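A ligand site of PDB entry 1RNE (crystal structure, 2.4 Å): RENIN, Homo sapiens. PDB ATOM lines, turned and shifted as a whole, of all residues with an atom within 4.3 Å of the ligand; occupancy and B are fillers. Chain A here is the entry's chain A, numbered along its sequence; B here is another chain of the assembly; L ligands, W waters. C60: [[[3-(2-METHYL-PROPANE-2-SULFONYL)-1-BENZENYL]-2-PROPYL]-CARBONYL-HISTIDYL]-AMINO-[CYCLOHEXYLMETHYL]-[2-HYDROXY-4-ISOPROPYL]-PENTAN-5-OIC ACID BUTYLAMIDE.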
ATOM      1  N   GLN A  19     -10.461   9.387 -23.743  1.00  0.00           N
ATOM      2  CA  GLN A  19     -11.160  10.675 -23.758  1.00  0.00           C
ATOM      3  C   GLN A  19     -12.419  10.483 -24.498  1.00  0.00           C
ATOM      4  O   GLN A  19     -12.380  10.178 -25.678  1.00  0.00           O
ATOM      5  CB  GLN A  19     -10.408  11.763 -24.528  1.00  0.00           C
ATOM      6  CG  GLN A  19      -9.007  11.966 -23.949  1.00  0.00           C
ATOM      7  CD  GLN A  19      -8.229  13.073 -24.624  1.00  0.00           C
ATOM      8  OE1 GLN A  19      -7.014  13.178 -24.399  1.00  0.00           O
ATOM      9  NE2 GLN A  19      -8.896  13.901 -25.434  1.00  0.00           N
ATOM     10  N   VAL A  36     -15.876  17.013 -21.874  1.00  0.00           N
ATOM     11  CA  VAL A  36     -16.004  15.710 -21.250  1.00  0.00           C
ATOM     12  C   VAL A  36     -17.129  15.940 -20.255  1.00  0.00           C
ATOM     13  O   VAL A  36     -17.271  17.060 -19.776  1.00  0.00           O
ATOM     14  CB  VAL A  36     -14.694  15.421 -20.557  1.00  0.00           C
ATOM     15  CG1 VAL A  36     -14.788  14.405 -19.460  1.00  0.00           C
ATOM     16  CG2 VAL A  36     -13.707  15.017 -21.645  1.00  0.00           C
ATOM     17  N   ASP A  38     -18.179  15.045 -16.837  1.00  0.00           N
ATOM     18  CA  ASP A  38     -17.591  14.408 -15.658  1.00  0.00           C
ATOM     19  C   ASP A  38     -18.471  14.234 -14.444  1.00  0.00           C
ATOM     20  O   ASP A  38     -18.864  15.250 -13.866  1.00  0.00           O
ATOM     21  CB  ASP A  38     -16.415  15.346 -15.315  1.00  0.00           C
ATOM     22  CG  ASP A  38     -15.685  15.041 -14.047  1.00  0.00           C
ATOM     23  OD1 ASP A  38     -15.581  13.914 -13.602  1.00  0.00           O
ATOM     24  OD2 ASP A  38     -15.240  16.121 -13.470  1.00  0.00           O
ATOM     25  N   GLY A  40     -17.535  13.486 -11.697  1.00  0.00           N
ATOM     26  CA  GLY A  40     -16.667  13.722 -10.508  1.00  0.00           C
ATOM     27  C   GLY A  40     -16.564  15.182 -10.128  1.00  0.00           C
ATOM     28  O   GLY A  40     -15.883  15.501  -9.167  1.00  0.00           O
ATOM     29  N   SER A  41     -17.237  16.058 -10.894  1.00  0.00           N
ATOM     30  CA  SER A  41     -17.166  17.453 -10.560  1.00  0.00           C
ATOM     31  C   SER A  41     -18.446  18.188 -10.937  1.00  0.00           C
ATOM     32  O   SER A  41     -19.372  17.643 -11.530  1.00  0.00           O
ATOM     33  CB  SER A  41     -15.929  18.079 -11.101  1.00  0.00           C
ATOM     34  OG  SER A  41     -16.088  18.237 -12.493  1.00  0.00           O
ATOM     35  N   LEU A  81      -9.990  25.884 -10.166  1.00  0.00           N
ATOM     36  CA  LEU A  81     -10.460  24.527 -10.070  1.00  0.00           C
ATOM     37  C   LEU A  81      -9.327  23.531 -10.104  1.00  0.00           C
ATOM     38  O   LEU A  81      -8.686  23.335 -11.147  1.00  0.00           O
ATOM     39  CB  LEU A  81     -11.411  24.234 -11.208  1.00  0.00           C
ATOM     40  CG  LEU A  81     -12.402  25.352 -11.390  1.00  0.00           C
ATOM     41  CD1 LEU A  81     -12.702  25.558 -12.849  1.00  0.00           C
ATOM     42  CD2 LEU A  81     -13.698  24.874 -10.778  1.00  0.00           C
ATOM     43  N   ARG A  82      -9.089  22.935  -8.931  1.00  0.00           N
ATOM     44  CA  ARG A  82      -8.078  21.935  -8.713  1.00  0.00           C
ATOM     45  C   ARG A  82      -8.655  20.517  -8.957  1.00  0.00           C
ATOM     46  O   ARG A  82      -9.504  20.032  -8.235  1.00  0.00           O
ATOM     47  CB  ARG A  82      -7.308  21.967  -7.346  1.00  0.00           C
ATOM     48  CG  ARG A  82      -5.937  22.661  -7.179  1.00  0.00           C
ATOM     49  CD  ARG A  82      -5.826  23.287  -5.785  1.00  0.00           C
ATOM     50  NE  ARG A  82      -4.908  24.404  -5.792  1.00  0.00           N
ATOM     51  CZ  ARG A  82      -5.292  25.658  -5.971  1.00  0.00           C
ATOM     52  NH1 ARG A  82      -6.578  25.962  -6.118  1.00  0.00           N
ATOM     53  NH2 ARG A  82      -4.408  26.640  -5.980  1.00  0.00           N
ATOM     54  N   TYR A  83      -8.205  19.837  -9.993  1.00  0.00           N
ATOM     55  CA  TYR A  83      -8.639  18.484 -10.247  1.00  0.00           C
ATOM     56  C   TYR A  83      -7.548  17.473  -9.780  1.00  0.00           C
ATOM     57  O   TYR A  83      -6.465  17.866  -9.385  1.00  0.00           O
ATOM     58  CB  TYR A  83      -8.944  18.213 -11.733  1.00  0.00           C
ATOM     59  CG  TYR A  83     -10.052  19.013 -12.322  1.00  0.00           C
ATOM     60  CD1 TYR A  83     -11.346  18.522 -12.212  1.00  0.00           C
ATOM     61  CD2 TYR A  83      -9.836  20.212 -12.997  1.00  0.00           C
ATOM     62  CE1 TYR A  83     -12.444  19.175 -12.762  1.00  0.00           C
ATOM     63  CE2 TYR A  83     -10.926  20.880 -13.532  1.00  0.00           C
ATOM     64  CZ  TYR A  83     -12.222  20.370 -13.415  1.00  0.00           C
ATOM     65  OH  TYR A  83     -13.320  21.049 -13.950  1.00  0.00           O
ATOM     66  N   SER A  84      -7.836  16.155  -9.847  1.00  0.00           N
ATOM     67  CA  SER A  84      -6.875  15.146  -9.483  1.00  0.00           C
ATOM     68  C   SER A  84      -5.628  15.399 -10.333  1.00  0.00           C
ATOM     69  O   SER A  84      -4.505  15.381  -9.879  1.00  0.00           O
ATOM     70  CB  SER A  84      -7.483  13.793  -9.801  1.00  0.00           C
ATOM     71  OG  SER A  84      -8.291  13.470  -8.685  1.00  0.00           O
ATOM     72  N   THR A  85      -5.908  15.706 -11.585  1.00  0.00           N
ATOM     73  CA  THR A  85      -4.888  16.006 -12.535  1.00  0.00           C
ATOM     74  C   THR A  85      -5.150  17.357 -13.193  1.00  0.00           C
ATOM     75  O   THR A  85      -6.035  17.474 -14.043  1.00  0.00           O
ATOM     76  CB  THR A  85      -4.881  14.991 -13.683  1.00  0.00           C
ATOM     77  OG1 THR A  85      -6.061  15.112 -14.447  1.00  0.00           O
ATOM     78  CG2 THR A  85      -4.598  13.558 -13.289  1.00  0.00           C
ATOM     79  N   PRO A 118      -1.824  18.706 -17.671  1.00  0.00           N
ATOM     80  CA  PRO A 118      -2.194  17.724 -18.676  1.00  0.00           C
ATOM     81  C   PRO A 118      -2.958  18.257 -19.853  1.00  0.00           C
ATOM     82  O   PRO A 118      -3.287  17.477 -20.754  1.00  0.00           O
ATOM     83  CB  PRO A 118      -3.282  16.902 -17.970  1.00  0.00           C
ATOM     84  CG  PRO A 118      -3.993  17.924 -17.119  1.00  0.00           C
ATOM     85  CD  PRO A 118      -2.894  18.879 -16.694  1.00  0.00           C
ATOM     86  N   PHE A 119      -3.326  19.542 -19.878  1.00  0.00           N
ATOM     87  CA  PHE A 119      -4.135  20.043 -21.038  1.00  0.00           C
ATOM     88  C   PHE A 119      -3.632  19.893 -22.463  1.00  0.00           C
ATOM     89  O   PHE A 119      -4.455  19.950 -23.375  1.00  0.00           O
ATOM     90  CB  PHE A 119      -4.949  21.340 -20.819  1.00  0.00           C
ATOM     91  CG  PHE A 119      -5.749  21.205 -19.559  1.00  0.00           C
ATOM     92  CD1 PHE A 119      -6.953  20.516 -19.650  1.00  0.00           C
ATOM     93  CD2 PHE A 119      -5.338  21.624 -18.283  1.00  0.00           C
ATOM     94  CE1 PHE A 119      -7.758  20.307 -18.512  1.00  0.00           C
ATOM     95  CE2 PHE A 119      -6.121  21.413 -17.142  1.00  0.00           C
ATOM     96  CZ  PHE A 119      -7.349  20.733 -17.248  1.00  0.00           C
ATOM     97  N   LEU A 121      -2.544  17.296 -23.665  1.00  0.00           N
ATOM     98  CA  LEU A 121      -2.897  15.971 -24.084  1.00  0.00           C
ATOM     99  C   LEU A 121      -4.391  15.974 -24.440  1.00  0.00           C
ATOM    100  O   LEU A 121      -4.936  15.048 -25.009  1.00  0.00           O
ATOM    101  CB  LEU A 121      -2.719  14.964 -22.922  1.00  0.00           C
ATOM    102  CG  LEU A 121      -1.309  14.983 -22.349  1.00  0.00           C
ATOM    103  CD1 LEU A 121      -1.271  13.982 -21.221  1.00  0.00           C
ATOM    104  CD2 LEU A 121      -0.371  14.529 -23.448  1.00  0.00           C
ATOM    105  N   ALA A 122      -5.065  17.059 -24.103  1.00  0.00           N
ATOM    106  CA  ALA A 122      -6.484  17.098 -24.298  1.00  0.00           C
ATOM    107  C   ALA A 122      -7.058  17.176 -25.642  1.00  0.00           C
ATOM    108  O   ALA A 122      -6.774  18.094 -26.396  1.00  0.00           O
ATOM    109  CB  ALA A 122      -7.119  18.165 -23.413  1.00  0.00           C
ATOM    110  N   PHE A 124     -10.336  17.533 -26.058  1.00  0.00           N
ATOM    111  CA  PHE A 124     -11.539  18.285 -25.800  1.00  0.00           C
ATOM    112  C   PHE A 124     -11.131  19.664 -25.420  1.00  0.00           C
ATOM    113  O   PHE A 124      -9.949  19.901 -25.164  1.00  0.00           O
ATOM    114  CB  PHE A 124     -12.294  17.578 -24.637  1.00  0.00           C
ATOM    115  CG  PHE A 124     -11.454  17.262 -23.421  1.00  0.00           C
ATOM    116  CD1 PHE A 124     -10.733  16.058 -23.372  1.00  0.00           C
ATOM    117  CD2 PHE A 124     -11.388  18.154 -22.355  1.00  0.00           C
ATOM    118  CE1 PHE A 124      -9.967  15.724 -22.267  1.00  0.00           C
ATOM    119  CE2 PHE A 124     -10.616  17.841 -21.247  1.00  0.00           C
ATOM    120  CZ  PHE A 124      -9.934  16.636 -21.216  1.00  0.00           C
ATOM    121  N   VAL A 127     -14.775  21.041 -19.889  1.00  0.00           N
ATOM    122  CA  VAL A 127     -15.529  20.167 -19.024  1.00  0.00           C
ATOM    123  C   VAL A 127     -16.931  20.706 -18.623  1.00  0.00           C
ATOM    124  O   VAL A 127     -17.184  21.892 -18.364  1.00  0.00           O
ATOM    125  CB  VAL A 127     -14.742  19.876 -17.693  1.00  0.00           C
ATOM    126  CG1 VAL A 127     -15.412  18.793 -16.845  1.00  0.00           C
ATOM    127  CG2 VAL A 127     -13.274  19.522 -17.839  1.00  0.00           C
ATOM    128  N   GLN A 135     -20.277  19.769  -4.671  1.00  0.00           N
ATOM    129  CA  GLN A 135     -18.894  19.663  -5.214  1.00  0.00           C
ATOM    130  C   GLN A 135     -18.474  20.882  -6.066  1.00  0.00           C
ATOM    131  O   GLN A 135     -17.364  21.025  -6.571  1.00  0.00           O
ATOM    132  CB  GLN A 135     -18.715  18.376  -6.039  1.00  0.00           C
ATOM    133  CG  GLN A 135     -18.901  17.051  -5.284  1.00  0.00           C
ATOM    134  CD  GLN A 135     -18.859  15.925  -6.280  1.00  0.00           C
ATOM    135  OE1 GLN A 135     -17.728  15.398  -6.496  1.00  0.00           O
ATOM    136  NE2 GLN A 135     -20.068  15.606  -6.847  1.00  0.00           N
ATOM    137  N   ILE A 137     -17.553  24.329  -7.070  1.00  0.00           N
ATOM    138  CA  ILE A 137     -16.737  25.355  -6.573  1.00  0.00           C
ATOM    139  C   ILE A 137     -17.520  26.653  -6.714  1.00  0.00           C
ATOM    140  O   ILE A 137     -18.122  26.921  -7.733  1.00  0.00           O
ATOM    141  CB  ILE A 137     -15.409  25.407  -7.297  1.00  0.00           C
ATOM    142  CG1 ILE A 137     -14.378  24.564  -6.551  1.00  0.00           C
ATOM    143  CG2 ILE A 137     -14.953  26.867  -7.250  1.00  0.00           C
ATOM    144  CD1 ILE A 137     -14.978  23.374  -5.802  1.00  0.00           C
ATOM    145  N   LEU A 224     -16.048   5.968  -6.195  1.00  0.00           N
ATOM    146  CA  LEU A 224     -16.739   7.083  -6.800  1.00  0.00           C
ATOM    147  C   LEU A 224     -16.939   6.652  -8.248  1.00  0.00           C
ATOM    148  O   LEU A 224     -15.984   6.154  -8.848  1.00  0.00           O
ATOM    149  CB  LEU A 224     -15.879   8.289  -6.787  1.00  0.00           C
ATOM    150  CG  LEU A 224     -16.707   9.521  -6.822  1.00  0.00           C
ATOM    151  CD1 LEU A 224     -15.967  10.542  -5.968  1.00  0.00           C
ATOM    152  CD2 LEU A 224     -16.688  10.017  -8.251  1.00  0.00           C
ATOM    153  N   ASP A 226     -16.823   7.648 -11.652  1.00  0.00           N
ATOM    154  CA  ASP A 226     -16.400   8.923 -12.343  1.00  0.00           C
ATOM    155  C   ASP A 226     -16.194   8.808 -13.836  1.00  0.00           C
ATOM    156  O   ASP A 226     -15.263   8.158 -14.237  1.00  0.00           O
ATOM    157  CB  ASP A 226     -15.125   9.392 -11.623  1.00  0.00           C
ATOM    158  CG  ASP A 226     -14.485  10.648 -12.073  1.00  0.00           C
ATOM    159  OD1 ASP A 226     -15.072  11.201 -13.126  1.00  0.00           O
ATOM    160  OD2 ASP A 226     -13.506  11.083 -11.502  1.00  0.00           O
ATOM    161  N   GLY A 228     -15.344  11.119 -15.843  1.00  0.00           N
ATOM    162  CA  GLY A 228     -14.319  11.935 -16.376  1.00  0.00           C
ATOM    163  C   GLY A 228     -12.917  11.473 -15.995  1.00  0.00           C
ATOM    164  O   GLY A 228     -11.977  12.243 -16.167  1.00  0.00           O
ATOM    165  N   ALA A 229     -12.779  10.259 -15.449  1.00  0.00           N
ATOM    166  CA  ALA A 229     -11.488   9.609 -15.068  1.00  0.00           C
ATOM    167  C   ALA A 229     -11.284   8.534 -16.133  1.00  0.00           C
ATOM    168  O   ALA A 229     -12.166   7.698 -16.256  1.00  0.00           O
ATOM    169  CB  ALA A 229     -11.604   8.899 -13.739  1.00  0.00           C
ATOM    170  N   SER A 230     -10.192   8.542 -16.915  1.00  0.00           N
ATOM    171  CA  SER A 230      -9.969   7.531 -17.974  1.00  0.00           C
ATOM    172  C   SER A 230      -9.707   6.102 -17.482  1.00  0.00           C
ATOM    173  O   SER A 230      -9.942   5.122 -18.185  1.00  0.00           O
ATOM    174  CB  SER A 230      -8.716   7.918 -18.742  1.00  0.00           C
ATOM    175  OG  SER A 230      -8.622   9.303 -19.108  1.00  0.00           O
ATOM    176  N   TYR A 231      -9.148   6.004 -16.294  1.00  0.00           N
ATOM    177  CA  TYR A 231      -8.808   4.696 -15.758  1.00  0.00           C
ATOM    178  C   TYR A 231      -9.572   4.397 -14.465  1.00  0.00           C
ATOM    179  O   TYR A 231     -10.372   5.173 -14.054  1.00  0.00           O
ATOM    180  CB  TYR A 231      -7.296   4.690 -15.376  1.00  0.00           C
ATOM    181  CG  TYR A 231      -6.282   4.838 -16.492  1.00  0.00           C
ATOM    182  CD1 TYR A 231      -6.702   4.669 -17.815  1.00  0.00           C
ATOM    183  CD2 TYR A 231      -4.938   5.040 -16.214  1.00  0.00           C
ATOM    184  CE1 TYR A 231      -5.804   4.754 -18.876  1.00  0.00           C
ATOM    185  CE2 TYR A 231      -4.026   5.135 -17.273  1.00  0.00           C
ATOM    186  CZ  TYR A 231      -4.469   4.985 -18.581  1.00  0.00           C
ATOM    187  OH  TYR A 231      -3.557   5.055 -19.588  1.00  0.00           O
ATOM    188  N   SER A 233      -9.187   3.935 -10.470  1.00  0.00           N
ATOM    189  CA  SER A 233      -8.251   4.474  -9.521  1.00  0.00           C
ATOM    190  C   SER A 233      -8.500   3.818  -8.176  1.00  0.00           C
ATOM    191  O   SER A 233      -9.551   3.283  -7.860  1.00  0.00           O
ATOM    192  CB  SER A 233      -8.425   6.022  -9.513  1.00  0.00           C
ATOM    193  OG  SER A 233      -8.602   6.508  -8.230  1.00  0.00           O
ATOM    194  N   HIS A 301      -4.636   3.016 -12.175  1.00  0.00           N
ATOM    195  CA  HIS A 301      -3.463   3.671 -11.670  1.00  0.00           C
ATOM    196  C   HIS A 301      -3.754   4.156 -10.306  1.00  0.00           C
ATOM    197  O   HIS A 301      -4.832   3.913  -9.830  1.00  0.00           O
ATOM    198  CB  HIS A 301      -2.918   4.751 -12.599  1.00  0.00           C
ATOM    199  CG  HIS A 301      -3.869   5.845 -12.835  1.00  0.00           C
ATOM    200  ND1 HIS A 301      -3.445   7.080 -13.269  1.00  0.00           N
ATOM    201  CD2 HIS A 301      -5.207   5.893 -12.663  1.00  0.00           C
ATOM    202  CE1 HIS A 301      -4.507   7.866 -13.358  1.00  0.00           C
ATOM    203  NE2 HIS A 301      -5.582   7.177 -12.999  1.00  0.00           N
ATOM    204  N   MET A 303      -4.407   6.912  -7.246  1.00  0.00           N
ATOM    205  CA  MET A 303      -4.859   8.271  -7.025  1.00  0.00           C
ATOM    206  C   MET A 303      -5.365   8.470  -5.613  1.00  0.00           C
ATOM    207  O   MET A 303      -6.364   7.894  -5.239  1.00  0.00           O
ATOM    208  CB  MET A 303      -5.971   8.703  -7.941  1.00  0.00           C
ATOM    209  CG  MET A 303      -5.403   9.185  -9.208  1.00  0.00           C
ATOM    210  SD  MET A 303      -4.711  10.827  -9.042  1.00  0.00           S
ATOM    211  CE  MET A 303      -4.436  10.653 -10.837  1.00  0.00           C
ATOM    212  N   ILE A 305      -7.281  10.541  -3.304  1.00  0.00           N
ATOM    213  CA  ILE A 305      -8.294  11.577  -3.330  1.00  0.00           C
ATOM    214  C   ILE A 305      -8.471  11.996  -1.871  1.00  0.00           C
ATOM    215  O   ILE A 305      -8.798  11.168  -0.991  1.00  0.00           O
ATOM    216  CB  ILE A 305      -9.566  11.050  -3.967  1.00  0.00           C
ATOM    217  CG1 ILE A 305      -9.225  10.763  -5.386  1.00  0.00           C
ATOM    218  CG2 ILE A 305     -10.592  12.162  -4.054  1.00  0.00           C
ATOM    219  CD1 ILE A 305     -10.170   9.723  -5.905  1.00  0.00           C
ATOM    220  N   ALA A 314     -12.068   4.861  -7.791  1.00  0.00           N
ATOM    221  CA  ALA A 314     -12.744   5.611  -8.799  1.00  0.00           C
ATOM    222  C   ALA A 314     -12.928   4.722  -9.962  1.00  0.00           C
ATOM    223  O   ALA A 314     -11.986   4.250 -10.554  1.00  0.00           O
ATOM    224  CB  ALA A 314     -12.159   6.968  -9.099  1.00  0.00           C
ATOM    225  N   LEU B 117       1.678  11.085 -24.402  1.00  0.00           N
ATOM    226  CA  LEU B 117       2.224  11.409 -23.108  1.00  0.00           C
ATOM    227  C   LEU B 117       3.562  10.693 -23.118  1.00  0.00           C
ATOM    228  O   LEU B 117       3.614   9.471 -23.273  1.00  0.00           O
ATOM    229  CB  LEU B 117       1.313  10.860 -22.006  1.00  0.00           C
ATOM    230  CG  LEU B 117       1.841  11.035 -20.594  1.00  0.00           C
ATOM    231  CD1 LEU B 117       1.882  12.520 -20.319  1.00  0.00           C
ATOM    232  CD2 LEU B 117       0.873  10.402 -19.601  1.00  0.00           C
ATOM    233  N   PHE B 253       1.461  14.713 -10.678  1.00  0.00           N
ATOM    234  CA  PHE B 253       2.513  15.122 -11.516  1.00  0.00           C
ATOM    235  C   PHE B 253       3.686  15.924 -10.920  1.00  0.00           C
ATOM    236  O   PHE B 253       4.641  16.189 -11.654  1.00  0.00           O
ATOM    237  CB  PHE B 253       1.836  16.017 -12.566  1.00  0.00           C
ATOM    238  CG  PHE B 253       0.806  15.421 -13.561  1.00  0.00           C
ATOM    239  CD1 PHE B 253       1.056  14.287 -14.348  1.00  0.00           C
ATOM    240  CD2 PHE B 253      -0.397  16.101 -13.763  1.00  0.00           C
ATOM    241  CE1 PHE B 253       0.118  13.825 -15.263  1.00  0.00           C
ATOM    242  CE2 PHE B 253      -1.341  15.668 -14.684  1.00  0.00           C
ATOM    243  CZ  PHE B 253      -1.081  14.523 -15.438  1.00  0.00           C
HETATM  244  CS1 C60 L   1      -3.612  10.002 -17.682  1.00  0.00           C
HETATM  245  CS2 C60 L   1      -4.357   8.666 -17.904  1.00  0.00           C
HETATM  246  CS3 C60 L   1      -2.278   9.747 -16.941  1.00  0.00           C
HETATM  247  CS4 C60 L   1      -3.273  10.738 -18.975  1.00  0.00           C
HETATM  248  SS  C60 L   1      -4.611  11.067 -16.782  1.00  0.00           S
HETATM  249  OS1 C60 L   1      -3.914  12.315 -16.704  1.00  0.00           O
HETATM  250  OS2 C60 L   1      -4.818  10.611 -15.490  1.00  0.00           O
HETATM  251  CNF C60 L   1      -6.136  11.198 -17.487  1.00  0.00           C
HETATM  252  CAF C60 L   1      -6.859  12.280 -16.715  1.00  0.00           C
HETATM  253  CBF C60 L   1      -7.908  12.825 -17.589  1.00  0.00           C
HETATM  254  C1F C60 L   1      -7.361  13.604 -18.745  1.00  0.00           C
HETATM  255  C2F C60 L   1      -7.315  12.934 -19.932  1.00  0.00           C
HETATM  256  C3F C60 L   1      -6.830  13.601 -21.063  1.00  0.00           C
HETATM  257  C4F C60 L   1      -6.427  14.947 -20.995  1.00  0.00           C
HETATM  258  C5F C60 L   1      -6.497  15.643 -19.806  1.00  0.00           C
HETATM  259  C6F C60 L   1      -6.980  14.969 -18.662  1.00  0.00           C
HETATM  260  CF  C60 L   1      -7.734  11.720 -15.692  1.00  0.00           C
HETATM  261  OF  C60 L   1      -8.349  10.724 -15.966  1.00  0.00           O
HETATM  262  NH  C60 L   1      -7.822  12.437 -14.602  1.00  0.00           N
HETATM  263  CAH C60 L   1      -8.650  12.056 -13.539  1.00  0.00           C
HETATM  264  CBH C60 L   1      -7.855  11.356 -12.404  1.00  0.00           C
HETATM  265  C1H C60 L   1      -8.597  10.397 -11.441  1.00  0.00           C
HETATM  266  N1H C60 L   1      -9.143  10.790 -10.193  1.00  0.00           N
HETATM  267  C2H C60 L   1      -8.829   9.074 -11.563  1.00  0.00           C
HETATM  268  N2H C60 L   1      -9.510   8.667 -10.428  1.00  0.00           N
HETATM  269  C3H C60 L   1      -9.683   9.708  -9.634  1.00  0.00           C
HETATM  270  CH  C60 L   1      -9.268  13.337 -13.047  1.00  0.00           C
HETATM  271  OH  C60 L   1      -8.657  14.172 -12.377  1.00  0.00           O
HETATM  272  NC  C60 L   1     -10.533  13.429 -13.399  1.00  0.00           N
HETATM  273  CAC C60 L   1     -11.400  14.544 -13.048  1.00  0.00           C
HETATM  274  CBC C60 L   1     -12.290  14.896 -14.210  1.00  0.00           C
HETATM  275  C1C C60 L   1     -11.394  15.193 -15.367  1.00  0.00           C
HETATM  276  C2C C60 L   1     -12.158  15.795 -16.530  1.00  0.00           C
HETATM  277  C3C C60 L   1     -11.166  15.944 -17.681  1.00  0.00           C
HETATM  278  C4C C60 L   1     -10.138  17.021 -17.330  1.00  0.00           C
HETATM  279  C5C C60 L   1      -9.500  16.799 -15.947  1.00  0.00           C
HETATM  280  C6C C60 L   1     -10.447  16.242 -14.851  1.00  0.00           C
HETATM  281  CC  C60 L   1     -12.327  14.346 -11.830  1.00  0.00           C
HETATM  282  OC  C60 L   1     -13.418  13.468 -12.091  1.00  0.00           O
HETATM  283  CNV C60 L   1     -11.565  13.968 -10.576  1.00  0.00           C
HETATM  284  CAV C60 L   1     -12.359  14.370  -9.363  1.00  0.00           C
HETATM  285  CBV C60 L   1     -11.985  13.533  -8.129  1.00  0.00           C
HETATM  286  C1V C60 L   1     -12.307  14.330  -6.923  1.00  0.00           C
HETATM  287  C2V C60 L   1     -12.827  12.298  -7.973  1.00  0.00           C
HETATM  288  CV  C60 L   1     -12.186  15.835  -9.035  1.00  0.00           C
HETATM  289  OV  C60 L   1     -11.123  16.397  -9.241  1.00  0.00           O
HETATM  290  NT  C60 L   1     -13.280  16.374  -8.491  1.00  0.00           N
HETATM  291  C1T C60 L   1     -13.489  17.680  -7.961  1.00  0.00           C
HETATM  292  C2T C60 L   1     -13.291  18.770  -8.931  1.00  0.00           C
HETATM  293  C3T C60 L   1     -13.595  20.030  -8.137  1.00  0.00           C
HETATM  294  C4T C60 L   1     -13.010  21.209  -8.921  1.00  0.00           C
HETATM  295  O   HOH W   1      -9.592  16.806  -6.717  1.00  0.00           O
HETATM  296  O   HOH W   2      -7.601   8.236 -14.781  1.00  0.00           O
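OC of the ligand is in hydrogen-bond range of OD2 of Asp 226.
OC of the ligand lies within hydrogen-bond range of OD1 of Asp 38, 2.7 Å away.
The backbone carbonyl oxygen (O) of Gly 40 sits at hydrogen-bond distance from a nitrogen (NT) of the ligand, at 2.8 Å.
The backbone NH (N) of Ser 84 sits close to an oxygen (OH) of the ligand (3.3 Å).
OG of Ser 84 lies within hydrogen-bond range of N1H of the ligand (3.2 Å).
OG of Ser 233 sits close to N2H of the ligand, 3.2 Å away.
An oxygen (OF) of the ligand is in hydrogen-bond range of the backbone NH (N) of Ser 230.
The side-chain hydroxyl (OG) of Ser 230 is in hydrogen-bond range of an oxygen (OF) of the ligand, at 3.5 Å.
The backbone carbonyl oxygen of Gly 228 lies close to a nitrogen (NC) of the ligand (3.3 Å).
N of Thr 85 sits at hydrogen-bond distance from OH of the ligand (3.2 Å).
OG1 of Thr 85 is in hydrogen-bond range of NH of the ligand (3.2 Å).
The backbone NH of Gly 228 lies within hydrogen-bond range of the side-chain carboxylate of Asp 226 (2.7 Å).
The side-chain carboxylate (OD1) of Asp 226 sits at hydrogen-bond distance from the backbone NH (N) of Ala 229 (3.4 Å).
N of Gly 40 is in hydrogen-bond range of OD1 of Asp 38 (2.8 Å).
The side-chain carboxylate of Asp 38 is in hydrogen-bond range of the side-chain hydroxyl of Ser 41 (2.5 Å).
The backbone carbonyl oxygen (O) of Gly 40 sits close to the side-chain amide oxygen (OE1) of Gln 135, 3.2 Å away.
O of Ala 314 sits at hydrogen-bond distance from N of Ser 233, 2.8 Å away.
The side-chain amide oxygen (OE1) of Gln 19 sits close to the backbone carbonyl oxygen (O) of Leu 121, 2.9 Å away.
Residues that only touch the ligand: Gln 19, Tyr 83, Ala 314, Ala 229, Ser 41, His 301, Tyr 231, Ile 305, Arg 82, Phe 124, Phe 253 of chain B, Pro 118, Met 303 and Ala 122.
The nearest printed residue that does not touch the ligand is Val 127 (4.04 Å).
Water W2 lies within hydrogen-bond range of an oxygen (OF) of the ligand (2.9 Å), a ring nitrogen (NE2) of His 301 (2.9 Å), the backbone NH of Tyr 231 (3.1 Å) and the backbone NH of Ser 230 (3.4 Å).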
